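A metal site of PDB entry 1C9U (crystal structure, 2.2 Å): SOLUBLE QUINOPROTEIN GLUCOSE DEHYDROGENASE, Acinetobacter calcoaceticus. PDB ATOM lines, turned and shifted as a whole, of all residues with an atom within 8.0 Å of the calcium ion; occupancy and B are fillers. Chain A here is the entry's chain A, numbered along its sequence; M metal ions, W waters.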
ATOM      1  N   SER A 250     -11.944 -18.911   0.401  1.00  0.00           N
ATOM      2  CA  SER A 250     -12.177 -19.138  -1.013  1.00  0.00           C
ATOM      3  C   SER A 250     -12.033 -17.875  -1.845  1.00  0.00           C
ATOM      4  O   SER A 250     -11.716 -16.788  -1.383  1.00  0.00           O
ATOM      5  CB  SER A 250     -13.594 -19.723  -1.208  1.00  0.00           C
ATOM      6  OG  SER A 250     -14.571 -18.765  -0.859  1.00  0.00           O
ATOM      7  N   ASP A 251     -12.253 -18.072  -3.145  1.00  0.00           N
ATOM      8  CA  ASP A 251     -12.285 -17.011  -4.124  1.00  0.00           C
ATOM      9  C   ASP A 251     -11.078 -16.085  -4.153  1.00  0.00           C
ATOM     10  O   ASP A 251     -11.221 -14.864  -4.101  1.00  0.00           O
ATOM     11  CB  ASP A 251     -13.595 -16.213  -3.935  1.00  0.00           C
ATOM     12  CG  ASP A 251     -14.786 -17.088  -4.271  1.00  0.00           C
ATOM     13  OD1 ASP A 251     -15.008 -17.366  -5.470  1.00  0.00           O
ATOM     14  OD2 ASP A 251     -15.513 -17.507  -3.346  1.00  0.00           O
ATOM     15  N   GLU A 253      -8.686 -14.054  -6.327  1.00  0.00           N
ATOM     16  CA  GLU A 253      -9.096 -13.523  -7.619  1.00  0.00           C
ATOM     17  C   GLU A 253      -8.014 -12.953  -8.516  1.00  0.00           C
ATOM     18  O   GLU A 253      -6.947 -12.517  -8.111  1.00  0.00           O
ATOM     19  CB  GLU A 253     -10.116 -12.394  -7.369  1.00  0.00           C
ATOM     20  CG  GLU A 253     -11.384 -12.803  -6.659  1.00  0.00           C
ATOM     21  CD  GLU A 253     -12.171 -11.605  -6.144  1.00  0.00           C
ATOM     22  OE1 GLU A 253     -11.679 -10.466  -6.244  1.00  0.00           O
ATOM     23  OE2 GLU A 253     -13.288 -11.782  -5.616  1.00  0.00           O
ATOM     24  N   ASN A 267     -18.550  -8.038   1.243  1.00  0.00           N
ATOM     25  CA  ASN A 267     -19.885  -8.596   1.016  1.00  0.00           C
ATOM     26  C   ASN A 267     -19.868  -9.725  -0.009  1.00  0.00           C
ATOM     27  O   ASN A 267     -20.693 -10.629   0.037  1.00  0.00           O
ATOM     28  CB  ASN A 267     -20.839  -7.488   0.592  1.00  0.00           C
ATOM     29  CG  ASN A 267     -21.053  -6.494   1.715  1.00  0.00           C
ATOM     30  OD1 ASN A 267     -21.916  -6.698   2.563  1.00  0.00           O
ATOM     31  ND2 ASN A 267     -20.273  -5.423   1.719  1.00  0.00           N
ATOM     32  N   VAL A 268     -18.891  -9.676  -0.922  1.00  0.00           N
ATOM     33  CA  VAL A 268     -18.775 -10.688  -1.955  1.00  0.00           C
ATOM     34  C   VAL A 268     -17.355 -11.176  -2.153  1.00  0.00           C
ATOM     35  O   VAL A 268     -16.441 -10.412  -2.466  1.00  0.00           O
ATOM     36  CB  VAL A 268     -19.288 -10.173  -3.319  1.00  0.00           C
ATOM     37  CG1 VAL A 268     -19.332 -11.311  -4.325  1.00  0.00           C
ATOM     38  CG2 VAL A 268     -20.649  -9.522  -3.182  1.00  0.00           C
ATOM     39  N   ALA A 269     -17.195 -12.489  -2.056  1.00  0.00           N
ATOM     40  CA  ALA A 269     -15.916 -13.132  -2.330  1.00  0.00           C
ATOM     41  C   ALA A 269     -16.020 -13.821  -3.689  1.00  0.00           C
ATOM     42  O   ALA A 269     -16.808 -14.763  -3.814  1.00  0.00           O
ATOM     43  CB  ALA A 269     -15.574 -14.138  -1.240  1.00  0.00           C
ATOM     44  N   GLY A 270     -15.317 -13.330  -4.703  1.00  0.00           N
ATOM     45  CA  GLY A 270     -15.400 -13.915  -6.034  1.00  0.00           C
ATOM     46  C   GLY A 270     -16.651 -13.426  -6.758  1.00  0.00           C
ATOM     47  O   GLY A 270     -16.983 -12.247  -6.705  1.00  0.00           O
ATOM     48  N   TYR A 271     -17.332 -14.338  -7.451  1.00  0.00           N
ATOM     49  CA  TYR A 271     -18.571 -13.990  -8.139  1.00  0.00           C
ATOM     50  C   TYR A 271     -19.670 -13.748  -7.120  1.00  0.00           C
ATOM     51  O   TYR A 271     -19.556 -14.216  -5.988  1.00  0.00           O
ATOM     52  CB  TYR A 271     -18.993 -15.124  -9.084  1.00  0.00           C
ATOM     53  CG  TYR A 271     -17.900 -15.555 -10.034  1.00  0.00           C
ATOM     54  CD1 TYR A 271     -17.197 -16.737  -9.850  1.00  0.00           C
ATOM     55  CD2 TYR A 271     -17.569 -14.758 -11.122  1.00  0.00           C
ATOM     56  CE1 TYR A 271     -16.197 -17.121 -10.724  1.00  0.00           C
ATOM     57  CE2 TYR A 271     -16.569 -15.132 -12.006  1.00  0.00           C
ATOM     58  CZ  TYR A 271     -15.888 -16.310 -11.798  1.00  0.00           C
ATOM     59  OH  TYR A 271     -14.894 -16.675 -12.673  1.00  0.00           O
ATOM     60  N   LYS A 272     -20.696 -12.999  -7.503  1.00  0.00           N
ATOM     61  CA  LYS A 272     -21.843 -12.810  -6.603  1.00  0.00           C
ATOM     62  C   LYS A 272     -22.776 -13.996  -6.856  1.00  0.00           C
ATOM     63  O   LYS A 272     -23.728 -13.906  -7.637  1.00  0.00           O
ATOM     64  CB  LYS A 272     -22.556 -11.484  -6.801  1.00  0.00           C
ATOM     65  CG  LYS A 272     -23.735 -11.293  -5.849  1.00  0.00           C
ATOM     66  CD  LYS A 272     -24.620 -10.141  -6.286  1.00  0.00           C
ATOM     67  CE  LYS A 272     -23.902  -8.803  -6.220  1.00  0.00           C
ATOM     68  NZ  LYS A 272     -24.811  -7.675  -6.550  1.00  0.00           N
ATOM     69  N   ASP A 273     -22.445 -15.123  -6.251  1.00  0.00           N
ATOM     70  CA  ASP A 273     -23.161 -16.363  -6.490  1.00  0.00           C
ATOM     71  C   ASP A 273     -23.657 -17.070  -5.243  1.00  0.00           C
ATOM     72  O   ASP A 273     -24.243 -18.146  -5.356  1.00  0.00           O
ATOM     73  CB  ASP A 273     -22.225 -17.312  -7.250  1.00  0.00           C
ATOM     74  CG  ASP A 273     -20.863 -17.484  -6.599  1.00  0.00           C
ATOM     75  OD1 ASP A 273     -20.738 -17.248  -5.376  1.00  0.00           O
ATOM     76  OD2 ASP A 273     -19.909 -17.865  -7.308  1.00  0.00           O
ATOM     77  N   ASP A 274     -23.417 -16.493  -4.067  1.00  0.00           N
ATOM     78  CA  ASP A 274     -23.803 -17.110  -2.804  1.00  0.00           C
ATOM     79  C   ASP A 274     -23.306 -18.556  -2.751  1.00  0.00           C
ATOM     80  O   ASP A 274     -23.990 -19.432  -2.209  1.00  0.00           O
ATOM     81  CB  ASP A 274     -25.317 -17.108  -2.625  1.00  0.00           C
ATOM     82  CG  ASP A 274     -25.967 -15.752  -2.615  1.00  0.00           C
ATOM     83  OD1 ASP A 274     -25.274 -14.710  -2.625  1.00  0.00           O
ATOM     84  OD2 ASP A 274     -27.222 -15.724  -2.594  1.00  0.00           O
ATOM     85  N   SER A 275     -22.121 -18.801  -3.308  1.00  0.00           N
ATOM     86  CA  SER A 275     -21.589 -20.156  -3.363  1.00  0.00           C
ATOM     87  C   SER A 275     -20.304 -20.336  -2.570  1.00  0.00           C
ATOM     88  O   SER A 275     -19.219 -19.966  -3.021  1.00  0.00           O
ATOM     89  CB  SER A 275     -21.360 -20.539  -4.829  1.00  0.00           C
ATOM     90  OG  SER A 275     -21.237 -21.939  -4.956  1.00  0.00           O
ATOM     91  N   GLY A 276     -20.411 -20.939  -1.393  1.00  0.00           N
ATOM     92  CA  GLY A 276     -19.260 -21.235  -0.563  1.00  0.00           C
ATOM     93  C   GLY A 276     -18.808 -20.104   0.339  1.00  0.00           C
ATOM     94  O   GLY A 276     -17.819 -20.279   1.075  1.00  0.00           O
ATOM     95  N   TYR A 277     -19.467 -18.953   0.298  1.00  0.00           N
ATOM     96  CA  TYR A 277     -19.112 -17.836   1.142  1.00  0.00           C
ATOM     97  C   TYR A 277     -20.318 -16.956   1.452  1.00  0.00           C
ATOM     98  O   TYR A 277     -21.123 -16.631   0.583  1.00  0.00           O
ATOM     99  CB  TYR A 277     -17.987 -16.985   0.540  1.00  0.00           C
ATOM    100  CG  TYR A 277     -17.695 -15.693   1.277  1.00  0.00           C
ATOM    101  CD1 TYR A 277     -16.796 -15.652   2.328  1.00  0.00           C
ATOM    102  CD2 TYR A 277     -18.337 -14.520   0.923  1.00  0.00           C
ATOM    103  CE1 TYR A 277     -16.541 -14.471   2.999  1.00  0.00           C
ATOM    104  CE2 TYR A 277     -18.090 -13.332   1.581  1.00  0.00           C
ATOM    105  CZ  TYR A 277     -17.190 -13.312   2.619  1.00  0.00           C
ATOM    106  OH  TYR A 277     -16.944 -12.133   3.287  1.00  0.00           O
ATOM    107  N   ALA A 278     -20.370 -16.503   2.700  1.00  0.00           N
ATOM    108  CA  ALA A 278     -21.382 -15.553   3.143  1.00  0.00           C
ATOM    109  C   ALA A 278     -20.680 -14.530   4.024  1.00  0.00           C
ATOM    110  O   ALA A 278     -19.669 -14.883   4.636  1.00  0.00           O
ATOM    111  CB  ALA A 278     -22.505 -16.249   3.885  1.00  0.00           C
ATOM    112  N   ASN A 296     -16.108 -20.058   6.487  1.00  0.00           N
ATOM    113  CA  ASN A 296     -16.289 -19.071   5.435  1.00  0.00           C
ATOM    114  C   ASN A 296     -17.655 -18.396   5.422  1.00  0.00           C
ATOM    115  O   ASN A 296     -18.057 -17.850   4.401  1.00  0.00           O
ATOM    116  CB  ASN A 296     -16.001 -19.714   4.078  1.00  0.00           C
ATOM    117  CG  ASN A 296     -15.366 -18.759   3.085  1.00  0.00           C
ATOM    118  OD1 ASN A 296     -15.607 -18.822   1.885  1.00  0.00           O
ATOM    119  ND2 ASN A 296     -14.542 -17.850   3.597  1.00  0.00           N
ATOM    120  N   GLU A 309     -24.209 -12.637  -0.356  1.00  0.00           N
ATOM    121  CA  GLU A 309     -23.664 -11.668  -1.306  1.00  0.00           C
ATOM    122  C   GLU A 309     -24.790 -11.079  -2.146  1.00  0.00           C
ATOM    123  O   GLU A 309     -24.788  -9.927  -2.559  1.00  0.00           O
ATOM    124  CB  GLU A 309     -22.659 -12.349  -2.245  1.00  0.00           C
ATOM    125  CG  GLU A 309     -21.917 -13.495  -1.572  1.00  0.00           C
ATOM    126  CD  GLU A 309     -21.048 -14.285  -2.527  1.00  0.00           C
ATOM    127  OE1 GLU A 309     -21.532 -14.707  -3.601  1.00  0.00           O
ATOM    128  OE2 GLU A 309     -19.858 -14.497  -2.201  1.00  0.00           O
ATOM    129  N   PHE A 317     -20.424  -3.115  -8.694  1.00  0.00           N
ATOM    130  CA  PHE A 317     -19.704  -4.360  -8.413  1.00  0.00           C
ATOM    131  C   PHE A 317     -19.081  -4.920  -9.690  1.00  0.00           C
ATOM    132  O   PHE A 317     -19.746  -5.105 -10.716  1.00  0.00           O
ATOM    133  CB  PHE A 317     -20.589  -5.402  -7.735  1.00  0.00           C
ATOM    134  CG  PHE A 317     -19.928  -6.749  -7.613  1.00  0.00           C
ATOM    135  CD1 PHE A 317     -18.896  -6.966  -6.725  1.00  0.00           C
ATOM    136  CD2 PHE A 317     -20.360  -7.794  -8.415  1.00  0.00           C
ATOM    137  CE1 PHE A 317     -18.305  -8.210  -6.631  1.00  0.00           C
ATOM    138  CE2 PHE A 317     -19.768  -9.039  -8.321  1.00  0.00           C
ATOM    139  CZ  PHE A 317     -18.739  -9.246  -7.434  1.00  0.00           C
ATOM    140  N   PRO A 320     -14.574 -10.948 -10.667  1.00  0.00           N
ATOM    141  CA  PRO A 320     -13.255 -11.405 -11.062  1.00  0.00           C
ATOM    142  C   PRO A 320     -13.286 -12.050 -12.442  1.00  0.00           C
ATOM    143  O   PRO A 320     -14.342 -12.515 -12.878  1.00  0.00           O
ATOM    144  CB  PRO A 320     -12.907 -12.453 -10.005  1.00  0.00           C
ATOM    145  CG  PRO A 320     -14.225 -12.985  -9.569  1.00  0.00           C
ATOM    146  CD  PRO A 320     -15.201 -11.847  -9.656  1.00  0.00           C
ATOM    147  N   THR A 323     -11.492 -17.184 -10.494  1.00  0.00           N
ATOM    148  CA  THR A 323     -11.410 -17.417  -9.067  1.00  0.00           C
ATOM    149  C   THR A 323     -10.657 -18.714  -8.766  1.00  0.00           C
ATOM    150  O   THR A 323     -10.877 -19.725  -9.421  1.00  0.00           O
ATOM    151  CB  THR A 323     -12.793 -17.527  -8.387  1.00  0.00           C
ATOM    152  OG1 THR A 323     -13.527 -18.602  -9.006  1.00  0.00           O
ATOM    153  CG2 THR A 323     -13.583 -16.245  -8.499  1.00  0.00           C
ATOM    154  N   TYR A 325     -10.379 -20.680  -5.428  1.00  0.00           N
ATOM    155  CA  TYR A 325     -11.380 -21.273  -6.281  1.00  0.00           C
ATOM    156  C   TYR A 325     -12.770 -20.971  -5.743  1.00  0.00           C
ATOM    157  O   TYR A 325     -12.916 -20.512  -4.605  1.00  0.00           O
ATOM    158  CB  TYR A 325     -11.235 -22.818  -6.283  1.00  0.00           C
ATOM    159  CG  TYR A 325      -9.849 -23.203  -6.765  1.00  0.00           C
ATOM    160  CD1 TYR A 325      -8.815 -23.473  -5.891  1.00  0.00           C
ATOM    161  CD2 TYR A 325      -9.603 -23.270  -8.124  1.00  0.00           C
ATOM    162  CE1 TYR A 325      -7.558 -23.805  -6.354  1.00  0.00           C
ATOM    163  CE2 TYR A 325      -8.348 -23.604  -8.609  1.00  0.00           C
ATOM    164  CZ  TYR A 325      -7.333 -23.869  -7.721  1.00  0.00           C
ATOM    165  OH  TYR A 325      -6.082 -24.214  -8.186  1.00  0.00           O
ATOM    166  N   THR A 326     -13.794 -21.274  -6.540  1.00  0.00           N
ATOM    167  CA  THR A 326     -15.174 -21.141  -6.076  1.00  0.00           C
ATOM    168  C   THR A 326     -15.673 -22.557  -5.775  1.00  0.00           C
ATOM    169  O   THR A 326     -15.343 -23.485  -6.516  1.00  0.00           O
ATOM    170  CB  THR A 326     -16.089 -20.458  -7.097  1.00  0.00           C
ATOM    171  OG1 THR A 326     -15.611 -19.119  -7.336  1.00  0.00           O
ATOM    172  CG2 THR A 326     -17.517 -20.381  -6.580  1.00  0.00           C
ATOM    173  N   VAL A 327     -16.325 -22.720  -4.641  1.00  0.00           N
ATOM    174  CA  VAL A 327     -16.840 -24.033  -4.252  1.00  0.00           C
ATOM    175  C   VAL A 327     -18.307 -23.900  -3.853  1.00  0.00           C
ATOM    176  O   VAL A 327     -18.820 -22.779  -3.755  1.00  0.00           O
ATOM    177  CB  VAL A 327     -16.042 -24.663  -3.099  1.00  0.00           C
ATOM    178  CG1 VAL A 327     -14.623 -24.994  -3.543  1.00  0.00           C
ATOM    179  CG2 VAL A 327     -16.015 -23.743  -1.891  1.00  0.00           C
HETATM  180 CA    CA M   1     -18.883 -15.767  -4.237  1.00  0.00          CA
HETATM  181  O   HOH W   1     -17.553 -17.054  -6.011  1.00  0.00           O
HETATM  182  O   HOH W   2     -18.197 -17.617  -2.901  1.00  0.00           O
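The calcium ion is bound by O of Ala 269 (2.3 Å), water W2 (2.4 Å), O of Tyr 271 (2.4 Å), water W1 (2.6 Å), OE2 of Glu 309 (2.6 Å) and OD1 of Asp 273 (2.6 Å).
Slightly farther from the calcium ion lies the side-chain carboxylate (OE1) of Glu 309 (2.9 Å).
Water W2 bridges the backbone carbonyl oxygen of Ser 275 (2.6 Å) and the side-chain carboxylate of Asp 251 (2.7 Å).
Water W1 lies within hydrogen-bond range of OD1 of Asp 251 (2.6 Å), OD2 of Asp 273 (2.8 Å), N of Tyr 271 (3.1 Å) and OG1 of Thr 326 (3.1 Å).
The side-chain hydroxyl of Ser 250 is in hydrogen-bond range of the side-chain carboxylate of Asp 251, at 2.9 Å.
O of Tyr 325 sits at hydrogen-bond distance from N of Asp 251, 2.9 Å away.
OD1 of Asp 251 is in hydrogen-bond range of OG1 of Thr 326 (2.6 Å).
N of Ser 275 lies close to OD1 of Asp 273, at 2.9 Å.
The backbone NH (N) of Asp 274 is in hydrogen-bond range of the side-chain carboxylate (OE1) of Glu 309, at 2.6 Å.
Asp 251 touches the calcium ion (OD2 to CA, 3.9 Å).
Five residues have an atom within 4 Å of the calcium ion: Asp 251, Ala 269, Tyr 271, Asp 273 and Glu 309.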
